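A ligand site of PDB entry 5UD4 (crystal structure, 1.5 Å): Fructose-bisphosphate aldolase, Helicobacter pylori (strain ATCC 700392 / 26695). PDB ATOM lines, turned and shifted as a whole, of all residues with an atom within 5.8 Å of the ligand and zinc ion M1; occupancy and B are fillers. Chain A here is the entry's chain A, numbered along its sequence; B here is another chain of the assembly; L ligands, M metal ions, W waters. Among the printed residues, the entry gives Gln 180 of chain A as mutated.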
ATOM      1  N   ASN A  23     -17.013  12.626   7.796  1.00  0.00           N
ATOM      2  CA  ASN A  23     -17.319  14.024   7.578  1.00  0.00           C
ATOM      3  C   ASN A  23     -16.723  14.898   8.677  1.00  0.00           C
ATOM      4  O   ASN A  23     -16.598  14.480   9.836  1.00  0.00           O
ATOM      5  CB  ASN A  23     -18.818  14.241   7.539  1.00  0.00           C
ATOM      6  CG  ASN A  23     -19.430  13.724   6.272  1.00  0.00           C
ATOM      7  OD1 ASN A  23     -19.756  12.541   6.153  1.00  0.00           O
ATOM      8  ND2 ASN A  23     -19.568  14.612   5.287  1.00  0.00           N
ATOM      9  N   VAL A  25     -16.727  19.313   9.960  1.00  0.00           N
ATOM     10  CA  VAL A  25     -17.125  20.701   9.745  1.00  0.00           C
ATOM     11  C   VAL A  25     -16.183  21.678  10.417  1.00  0.00           C
ATOM     12  O   VAL A  25     -16.380  22.890  10.283  1.00  0.00           O
ATOM     13  CB  VAL A  25     -18.561  20.992  10.227  1.00  0.00           C
ATOM     14  CG1 VAL A  25     -19.540  20.005   9.629  1.00  0.00           C
ATOM     15  CG2 VAL A  25     -18.664  20.996  11.740  1.00  0.00           C
ATOM     16  N   GLN A  47     -14.118  13.756   4.352  1.00  0.00           N
ATOM     17  CA  GLN A  47     -15.069  14.325   3.416  1.00  0.00           C
ATOM     18  C   GLN A  47     -15.799  15.502   4.025  1.00  0.00           C
ATOM     19  O   GLN A  47     -15.956  15.629   5.238  1.00  0.00           O
ATOM     20  CB  GLN A  47     -16.046  13.285   2.841  1.00  0.00           C
ATOM     21  CG  GLN A  47     -16.887  12.536   3.804  1.00  0.00           C
ATOM     22  CD  GLN A  47     -17.802  11.519   3.101  1.00  0.00           C
ATOM     23  OE1 GLN A  47     -17.466  10.976   2.055  1.00  0.00           O
ATOM     24  NE2 GLN A  47     -18.925  11.268   3.702  1.00  0.00           N
ATOM     25  N   SER A  49     -19.220  17.994   3.139  1.00  0.00           N
ATOM     26  CA  SER A  49     -20.419  18.323   2.402  1.00  0.00           C
ATOM     27  C   SER A  49     -20.354  19.759   1.868  1.00  0.00           C
ATOM     28  O   SER A  49     -19.517  20.566   2.274  1.00  0.00           O
ATOM     29  CB  SER A  49     -21.624  18.194   3.299  1.00  0.00           C
ATOM     30  OG  SER A  49     -21.544  19.170   4.305  1.00  0.00           O
ATOM     31  N   GLU A  50     -21.277  20.081   0.967  1.00  0.00           N
ATOM     32  CA  GLU A  50     -21.377  21.460   0.495  1.00  0.00           C
ATOM     33  C   GLU A  50     -21.702  22.398   1.652  1.00  0.00           C
ATOM     34  O   GLU A  50     -21.192  23.525   1.707  1.00  0.00           O
ATOM     35  CB  GLU A  50     -22.403  21.564  -0.639  1.00  0.00           C
ATOM     36  CG  GLU A  50     -21.923  20.883  -1.924  1.00  0.00           C
ATOM     37  CD  GLU A  50     -22.896  20.942  -3.082  1.00  0.00           C
ATOM     38  OE1 GLU A  50     -22.405  20.781  -4.209  1.00  0.00           O
ATOM     39  OE2 GLU A  50     -24.130  21.114  -2.879  1.00  0.00           O
ATOM     40  N   GLY A  51     -22.504  21.944   2.621  1.00  0.00           N
ATOM     41  CA  GLY A  51     -22.822  22.800   3.748  1.00  0.00           C
ATOM     42  C   GLY A  51     -21.616  23.015   4.644  1.00  0.00           C
ATOM     43  O   GLY A  51     -21.387  24.122   5.140  1.00  0.00           O
ATOM     44  N   ALA A  52     -20.810  21.967   4.835  1.00  0.00           N
ATOM     45  CA  ALA A  52     -19.589  22.118   5.629  1.00  0.00           C
ATOM     46  C   ALA A  52     -18.627  23.064   4.935  1.00  0.00           C
ATOM     47  O   ALA A  52     -17.967  23.882   5.595  1.00  0.00           O
ATOM     48  CB  ALA A  52     -18.937  20.749   5.820  1.00  0.00           C
ATOM     49  N   ASP A  82     -18.386  15.575  -0.537  1.00  0.00           N
ATOM     50  CA  ASP A  82     -19.523  14.689  -0.280  1.00  0.00           C
ATOM     51  C   ASP A  82     -20.806  15.308  -0.828  1.00  0.00           C
ATOM     52  O   ASP A  82     -21.152  16.439  -0.507  1.00  0.00           O
ATOM     53  CB  ASP A  82     -19.600  14.445   1.223  1.00  0.00           C
ATOM     54  CG  ASP A  82     -20.711  13.516   1.627  1.00  0.00           C
ATOM     55  OD1 ASP A  82     -21.140  12.670   0.825  1.00  0.00           O
ATOM     56  OD2 ASP A  82     -21.138  13.640   2.797  1.00  0.00           O
ATOM     57  N   HIS A  83     -21.517  14.548  -1.670  1.00  0.00           N
ATOM     58  CA  HIS A  83     -22.795  14.984  -2.250  1.00  0.00           C
ATOM     59  C   HIS A  83     -22.691  16.372  -2.888  1.00  0.00           C
ATOM     60  O   HIS A  83     -23.451  17.290  -2.576  1.00  0.00           O
ATOM     61  CB  HIS A  83     -23.926  14.933  -1.223  1.00  0.00           C
ATOM     62  CG  HIS A  83     -24.437  13.553  -0.991  1.00  0.00           C
ATOM     63  ND1 HIS A  83     -23.734  12.625  -0.252  1.00  0.00           N
ATOM     64  CD2 HIS A  83     -25.541  12.914  -1.435  1.00  0.00           C
ATOM     65  CE1 HIS A  83     -24.402  11.486  -0.228  1.00  0.00           C
ATOM     66  NE2 HIS A  83     -25.496  11.631  -0.940  1.00  0.00           N
ATOM     67  N   GLU A 134     -23.859   8.182  -7.814  1.00  0.00           N
ATOM     68  CA  GLU A 134     -24.902   7.479  -7.077  1.00  0.00           C
ATOM     69  C   GLU A 134     -25.964   6.999  -8.059  1.00  0.00           C
ATOM     70  O   GLU A 134     -26.284   7.694  -9.027  1.00  0.00           O
ATOM     71  CB  GLU A 134     -25.542   8.388  -6.019  1.00  0.00           C
ATOM     72  CG  GLU A 134     -26.554   7.705  -5.104  1.00  0.00           C
ATOM     73  CD  GLU A 134     -26.807   8.463  -3.807  1.00  0.00           C
ATOM     74  OE1 GLU A 134     -26.296   9.595  -3.654  1.00  0.00           O
ATOM     75  OE2 GLU A 134     -27.487   7.899  -2.917  1.00  0.00           O
ATOM     76  N   SER A 179     -30.441   5.394   4.394  1.00  0.00           N
ATOM     77  CA  SER A 179     -30.723   6.814   4.250  1.00  0.00           C
ATOM     78  C   SER A 179     -29.900   7.552   5.285  1.00  0.00           C
ATOM     79  O   SER A 179     -29.481   6.981   6.292  1.00  0.00           O
ATOM     80  CB  SER A 179     -32.205   7.146   4.423  1.00  0.00           C
ATOM     81  OG  SER A 179     -32.676   6.660   5.666  1.00  0.00           O
ATOM     82  N   GLN A 180     -29.666   8.837   5.025  1.00  0.00           N
ATOM     83  CA  GLN A 180     -28.810   9.621   5.892  1.00  0.00           C
ATOM     84  C   GLN A 180     -29.567  10.032   7.158  1.00  0.00           C
ATOM     85  O   GLN A 180     -30.798  10.065   7.198  1.00  0.00           O
ATOM     86  CB  GLN A 180     -28.277  10.862   5.178  1.00  0.00           C
ATOM     87  CG  GLN A 180     -29.304  11.979   4.959  1.00  0.00           C
ATOM     88  CD  GLN A 180     -28.739  13.151   4.137  1.00  0.00           C
ATOM     89  OE1 GLN A 180     -28.397  12.989   2.963  1.00  0.00           O
ATOM     90  NE2 GLN A 180     -28.658  14.322   4.759  1.00  0.00           N
ATOM     91  N   GLY A 181     -28.805  10.317   8.205  1.00  0.00           N
ATOM     92  CA  GLY A 181     -29.381  10.800   9.441  1.00  0.00           C
ATOM     93  C   GLY A 181     -29.664   9.694  10.437  1.00  0.00           C
ATOM     94  O   GLY A 181     -29.370   8.509  10.249  1.00  0.00           O
ATOM     95  N   ALA A 182     -30.265  10.117  11.558  1.00  0.00           N
ATOM     96  CA  ALA A 182     -30.445   9.240  12.694  1.00  0.00           C
ATOM     97  C   ALA A 182     -31.657   8.327  12.565  1.00  0.00           C
ATOM     98  O   ALA A 182     -31.766   7.355  13.324  1.00  0.00           O
ATOM     99  CB  ALA A 182     -30.559  10.095  13.961  1.00  0.00           C
ATOM    100  N   LYS A 184     -33.128   5.971  10.246  1.00  0.00           N
ATOM    101  CA  LYS A 184     -32.927   5.204   9.019  1.00  0.00           C
ATOM    102  C   LYS A 184     -34.034   4.184   8.793  1.00  0.00           C
ATOM    103  O   LYS A 184     -34.408   3.914   7.646  1.00  0.00           O
ATOM    104  CB  LYS A 184     -31.580   4.487   9.033  1.00  0.00           C
ATOM    105  CG  LYS A 184     -30.379   5.414   9.131  1.00  0.00           C
ATOM    106  CD  LYS A 184     -29.068   4.651   9.023  1.00  0.00           C
ATOM    107  CE  LYS A 184     -27.890   5.528   9.405  1.00  0.00           C
ATOM    108  NZ  LYS A 184     -27.868   6.816   8.634  1.00  0.00           N
ATOM    109  N   LEU A 209     -21.199   3.011   0.495  1.00  0.00           N
ATOM    110  CA  LEU A 209     -22.413   2.958   1.302  1.00  0.00           C
ATOM    111  C   LEU A 209     -22.658   4.316   1.941  1.00  0.00           C
ATOM    112  O   LEU A 209     -21.841   4.801   2.749  1.00  0.00           O
ATOM    113  CB  LEU A 209     -22.335   1.885   2.395  1.00  0.00           C
ATOM    114  CG  LEU A 209     -23.640   1.589   3.139  1.00  0.00           C
ATOM    115  CD1 LEU A 209     -24.662   0.951   2.190  1.00  0.00           C
ATOM    116  CD2 LEU A 209     -23.382   0.669   4.334  1.00  0.00           C
ATOM    117  N   HIS A 210     -23.767   4.929   1.584  1.00  0.00           N
ATOM    118  CA  HIS A 210     -24.219   6.164   2.203  1.00  0.00           C
ATOM    119  C   HIS A 210     -25.074   5.840   3.426  1.00  0.00           C
ATOM    120  O   HIS A 210     -25.607   4.745   3.564  1.00  0.00           O
ATOM    121  CB  HIS A 210     -25.041   6.982   1.225  1.00  0.00           C
ATOM    122  CG  HIS A 210     -24.237   7.543   0.089  1.00  0.00           C
ATOM    123  ND1 HIS A 210     -24.824   8.210  -0.967  1.00  0.00           N
ATOM    124  CD2 HIS A 210     -22.919   7.490  -0.178  1.00  0.00           C
ATOM    125  CE1 HIS A 210     -23.872   8.582  -1.819  1.00  0.00           C
ATOM    126  NE2 HIS A 210     -22.709   8.181  -1.338  1.00  0.00           N
ATOM    127  N   GLY A 211     -25.207   6.816   4.324  1.00  0.00           N
ATOM    128  CA  GLY A 211     -26.087   6.678   5.472  1.00  0.00           C
ATOM    129  C   GLY A 211     -25.728   5.503   6.355  1.00  0.00           C
ATOM    130  O   GLY A 211     -26.588   4.739   6.795  1.00  0.00           O
ATOM    131  N   ALA A 212     -24.434   5.369   6.642  1.00  0.00           N
ATOM    132  CA  ALA A 212     -23.885   4.161   7.240  1.00  0.00           C
ATOM    133  C   ALA A 212     -23.591   4.295   8.739  1.00  0.00           C
ATOM    134  O   ALA A 212     -22.934   3.419   9.299  1.00  0.00           O
ATOM    135  CB  ALA A 212     -22.601   3.755   6.503  1.00  0.00           C
ATOM    136  N   SER A 213     -24.074   5.350   9.394  1.00  0.00           N
ATOM    137  CA  SER A 213     -23.900   5.407  10.841  1.00  0.00           C
ATOM    138  C   SER A 213     -24.681   4.271  11.505  1.00  0.00           C
ATOM    139  O   SER A 213     -25.728   3.825  11.015  1.00  0.00           O
ATOM    140  CB  SER A 213     -24.357   6.764  11.395  1.00  0.00           C
ATOM    141  OG  SER A 213     -23.348   7.751  11.187  1.00  0.00           O
ATOM    142  N   ASN A 253     -19.708   5.916   4.413  1.00  0.00           N
ATOM    143  CA  ASN A 253     -19.924   7.301   4.791  1.00  0.00           C
ATOM    144  C   ASN A 253     -20.487   7.378   6.204  1.00  0.00           C
ATOM    145  O   ASN A 253     -21.553   6.810   6.487  1.00  0.00           O
ATOM    146  CB  ASN A 253     -20.876   7.991   3.826  1.00  0.00           C
ATOM    147  CG  ASN A 253     -20.278   8.234   2.440  1.00  0.00           C
ATOM    148  OD1 ASN A 253     -19.352   7.559   2.010  1.00  0.00           O
ATOM    149  ND2 ASN A 253     -20.822   9.217   1.739  1.00  0.00           N
ATOM    150  N   THR A 254     -19.799   8.120   7.070  1.00  0.00           N
ATOM    151  CA  THR A 254     -20.065   8.142   8.513  1.00  0.00           C
ATOM    152  C   THR A 254     -19.989   9.573   9.022  1.00  0.00           C
ATOM    153  O   THR A 254     -18.923  10.210   8.966  1.00  0.00           O
ATOM    154  CB  THR A 254     -19.057   7.248   9.234  1.00  0.00           C
ATOM    155  OG1 THR A 254     -19.006   5.973   8.578  1.00  0.00           O
ATOM    156  CG2 THR A 254     -19.442   7.055  10.673  1.00  0.00           C
ATOM    157  N   ASP A 255     -21.107  10.075   9.535  1.00  0.00           N
ATOM    158  CA  ASP A 255     -21.207  11.459   9.999  1.00  0.00           C
ATOM    159  C   ASP A 255     -22.042  11.547  11.284  1.00  0.00           C
ATOM    160  O   ASP A 255     -21.541  11.994  12.320  1.00  0.00           O
ATOM    161  CB  ASP A 255     -21.791  12.325   8.858  1.00  0.00           C
ATOM    162  CG  ASP A 255     -21.777  13.828   9.153  1.00  0.00           C
ATOM    163  OD1 ASP A 255     -21.456  14.225  10.278  1.00  0.00           O
ATOM    164  OD2 ASP A 255     -22.084  14.630   8.231  1.00  0.00           O
ATOM    165  N   THR A 256     -23.279  11.058  11.245  1.00  0.00           N
ATOM    166  CA  THR A 256     -24.190  11.138  12.381  1.00  0.00           C
ATOM    167  C   THR A 256     -23.569  10.580  13.666  1.00  0.00           C
ATOM    168  O   THR A 256     -23.650  11.215  14.735  1.00  0.00           O
ATOM    169  CB  THR A 256     -25.480  10.390  12.050  1.00  0.00           C
ATOM    170  OG1 THR A 256     -26.176  11.112  11.033  1.00  0.00           O
ATOM    171  CG2 THR A 256     -26.397  10.258  13.254  1.00  0.00           C
ATOM    172  N   ASP A 257     -22.944   9.403  13.589  1.00  0.00           N
ATOM    173  CA  ASP A 257     -22.313   8.821  14.776  1.00  0.00           C
ATOM    174  C   ASP A 257     -21.309   9.792  15.387  1.00  0.00           C
ATOM    175  O   ASP A 257     -21.188   9.890  16.625  1.00  0.00           O
ATOM    176  CB  ASP A 257     -21.587   7.514  14.434  1.00  0.00           C
ATOM    177  CG  ASP A 257     -22.522   6.341  14.272  1.00  0.00           C
ATOM    178  OD1 ASP A 257     -23.730   6.482  14.550  1.00  0.00           O
ATOM    179  OD2 ASP A 257     -22.023   5.268  13.885  1.00  0.00           O
ATOM    180  N   ARG A 259     -21.246  13.119  15.145  1.00  0.00           N
ATOM    181  CA  ARG A 259     -21.922  14.285  15.717  1.00  0.00           C
ATOM    182  C   ARG A 259     -22.547  13.957  17.065  1.00  0.00           C
ATOM    183  O   ARG A 259     -22.449  14.746  18.011  1.00  0.00           O
ATOM    184  CB  ARG A 259     -23.025  14.775  14.788  1.00  0.00           C
ATOM    185  CG  ARG A 259     -22.644  15.189  13.421  1.00  0.00           C
ATOM    186  CD  ARG A 259     -23.916  15.657  12.684  1.00  0.00           C
ATOM    187  NE  ARG A 259     -23.686  15.758  11.258  1.00  0.00           N
ATOM    188  CZ  ARG A 259     -24.525  16.329  10.393  1.00  0.00           C
ATOM    189  NH1 ARG A 259     -25.658  16.897  10.807  1.00  0.00           N
ATOM    190  NH2 ARG A 259     -24.225  16.341   9.100  1.00  0.00           N
ATOM    191  N   ASP B 278     -26.168  18.773  15.243  1.00  0.00           N
ATOM    192  CA  ASP B 278     -25.390  19.358  14.157  1.00  0.00           C
ATOM    193  C   ASP B 278     -24.487  20.435  14.743  1.00  0.00           C
ATOM    194  O   ASP B 278     -24.976  21.436  15.274  1.00  0.00           O
ATOM    195  CB  ASP B 278     -26.329  19.937  13.108  1.00  0.00           C
ATOM    196  CG  ASP B 278     -25.619  20.574  11.916  1.00  0.00           C
ATOM    197  OD1 ASP B 278     -24.396  20.802  11.951  1.00  0.00           O
ATOM    198  OD2 ASP B 278     -26.311  20.856  10.921  1.00  0.00           O
ATOM    199  N   ARG B 280     -22.804  22.768  13.507  1.00  0.00           N
ATOM    200  CA  ARG B 280     -22.984  24.098  12.936  1.00  0.00           C
ATOM    201  C   ARG B 280     -24.147  24.847  13.567  1.00  0.00           C
ATOM    202  O   ARG B 280     -24.131  26.086  13.630  1.00  0.00           O
ATOM    203  CB  ARG B 280     -23.184  23.986  11.429  1.00  0.00           C
ATOM    204  CG  ARG B 280     -21.982  23.435  10.712  1.00  0.00           C
ATOM    205  CD  ARG B 280     -22.325  22.910   9.335  1.00  0.00           C
ATOM    206  NE  ARG B 280     -23.228  21.764   9.427  1.00  0.00           N
ATOM    207  CZ  ARG B 280     -23.392  20.826   8.495  1.00  0.00           C
ATOM    208  NH1 ARG B 280     -22.716  20.871   7.348  1.00  0.00           N
ATOM    209  NH2 ARG B 280     -24.243  19.841   8.697  1.00  0.00           N
HETATM  210  O1  LIG L   1     -24.505   9.141   6.723  1.00  0.00           O
HETATM  211  C1  LIG L   1     -23.554  10.105   6.298  1.00  0.00           C
HETATM  212  C2  LIG L   1     -23.541  10.300   4.789  1.00  0.00           C
HETATM  213  C3  LIG L   1     -22.964  11.581   4.269  1.00  0.00           C
HETATM  214  C4  LIG L   1     -24.009  12.717   4.171  1.00  0.00           C
HETATM  215  C5  LIG L   1     -23.560  13.888   5.029  1.00  0.00           C
HETATM  216  C6  LIG L   1     -24.485  15.097   4.951  1.00  0.00           C
HETATM  217  O2  LIG L   1     -23.283  18.540   6.000  1.00  0.00           O
HETATM  218  P1  LIG L   1     -24.509  17.684   5.686  1.00  0.00           P
HETATM  219  O3  LIG L   1     -25.156  17.907   4.315  1.00  0.00           O
HETATM  220  O4  LIG L   1     -25.500  17.670   6.832  1.00  0.00           O
HETATM  221  O5  LIG L   1     -23.848  16.193   5.619  1.00  0.00           O
HETATM  222  O6  LIG L   1     -23.530  13.446   6.397  1.00  0.00           O
HETATM  223  O7  LIG L   1     -25.305  12.281   4.608  1.00  0.00           O
HETATM  224  O8  LIG L   1     -22.439  11.341   2.973  1.00  0.00           O
HETATM  225  O9  LIG L   1     -23.948   9.458   3.990  1.00  0.00           O
HETATM  226  P2  LIG L   1     -24.971   9.054   8.275  1.00  0.00           P
HETATM  227  O10 LIG L   1     -25.983  10.163   8.431  1.00  0.00           O
HETATM  228  O11 LIG L   1     -25.517   7.666   8.446  1.00  0.00           O
HETATM  229  O12 LIG L   1     -23.687   9.271   9.033  1.00  0.00           O
HETATM  230 ZN    ZN M   1     -24.939  10.325   1.890  1.00  0.00          ZN
HETATM  231 ZN    ZN M   2     -26.944   9.528  -1.174  1.00  0.00          ZN
HETATM  232  O   HOH W   1     -24.644  16.645   1.993  1.00  0.00           O
HETATM  233  O   HOH W   2     -25.812  12.847   7.956  1.00  0.00           O
HETATM  234  O   HOH W   3     -27.566  17.578   3.864  1.00  0.00           O
HETATM  235  O   HOH W   4     -27.521  17.100   8.398  1.00  0.00           O
HETATM  236  O   HOH W   5     -21.273  17.365   7.591  1.00  0.00           O
HETATM  237  O   HOH W   6     -24.735  20.112   2.936  1.00  0.00           O
HETATM  238  O   HOH W   7     -27.314  19.510   7.068  1.00  0.00           O
HETATM  239  O   HOH W   8     -27.146   9.980   1.149  1.00  0.00           O
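NZ of Lys 184 is in salt-bridge range of O11 of the ligand, 2.5 Å away. OG of Ser 49 lies within hydrogen-bond range of O2 of the ligand, at 2.5 Å. The backbone NH of Asp 255 is in hydrogen-bond range of an oxygen (O12) of the ligand (2.7 Å). An oxygen (O6) of the ligand sits at hydrogen-bond distance from the side-chain carboxylate (OD2) of Asp 255. An oxygen (O8) of the ligand sits at hydrogen-bond distance from the side-chain carboxylate of Asp 82 (2.6 Å). The backbone NH (N) of Ser 213 lies within hydrogen-bond range of an oxygen (O11) of the ligand, 2.9 Å away. OG of Ser 213 is in hydrogen-bond range of O12 of the ligand (2.7 Å). The guanidinium group (NH1) of Arg 280 of chain B is in salt-bridge range of an oxygen (O2) of the ligand, at 2.8 Å. The backbone NH of Thr 256 is in hydrogen-bond range of an oxygen (O12) of the ligand, 2.9 Å away. The side-chain hydroxyl (OG1) of Thr 256 lies within hydrogen-bond range of an oxygen (O10) of the ligand. N of Gly 181 sits at hydrogen-bond distance from O10 of the ligand, 2.8 Å away. NH2 of Arg 259 is in salt-bridge range of O4 of the ligand, at 2.9 Å. ND2 of Asn 253 is in hydrogen-bond range of O8 of the ligand. The backbone NH of Gly 211 lies close to an oxygen (O1) of the ligand, 3.4 Å away. N of Ala 212 lies within hydrogen-bond range of O11 of the ligand.
Asn 23 touches the ligand. NE2 of Gln 47 touches O8 of the ligand, at 3.6 Å. His 83 touches the ligand (ND1 to O8, 3.7 Å). Gln 180 touches the ligand. CA of His 210 touches O9 of the ligand (3.8 Å). Thr 254 touches the ligand. The nearest printed residue that does not touch the ligand is Ala 52 (4.4 Å).
Zinc ion M1 is bound by water W8 (2.4 Å) and O9 of the ligand (2.5 Å). Zinc ion M1 has two donor atoms within binding distance.
The side-chain carboxylate of Asp 82 sits at hydrogen-bond distance from a ring nitrogen (ND1) of His 83 (2.8 Å). O of Gly 211 lies close to NZ of Lys 184, at 3.1 Å. OG of Ser 49 sits at hydrogen-bond distance from N of Ala 52 (2.9 Å). The side-chain amide nitrogen of Asn 23 lies within hydrogen-bond range of the side-chain carboxylate of Asp 82, at 3.1 Å. The backbone carbonyl oxygen of Asn 253 lies within hydrogen-bond range of the backbone NH of Ala 212 (3.2 Å). The side-chain amide nitrogen (ND2) of Asn 253 lies close to the side-chain amide nitrogen (NE2) of Gln 47, 3.4 Å away. O of Leu 209 is in hydrogen-bond range of N of Asn 253 (2.9 Å). The side-chain amide nitrogen (NE2) of Gln 47 is in hydrogen-bond range of the side-chain amide oxygen (OD1) of Asn 23, 2.9 Å away.
Water W7 bridges O4 of the ligand (2.6 Å) and NH2 of Arg 280 of chain B (3.5 Å). Water W4 lies within hydrogen-bond range of an oxygen (O4) of the ligand (2.6 Å) and the guanidinium group of Arg 259 (3.1 Å). Water W6 lies within hydrogen-bond range of an oxygen (O3) of the ligand (2.6 Å) and the backbone NH (N) of Gly 51 (2.9 Å). Water W5 lies within hydrogen-bond range of O2 of the ligand, OD2 of Asp 255 and NH2 of Arg 259.
Residues that only touch zinc ion M1: His 83 and His 210. Of the 28 residues printed, 2 come within 4 Å of zinc ion M1. The nearest printed residue that does not touch zinc ion M1 is Asn 253 (4.3 Å).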
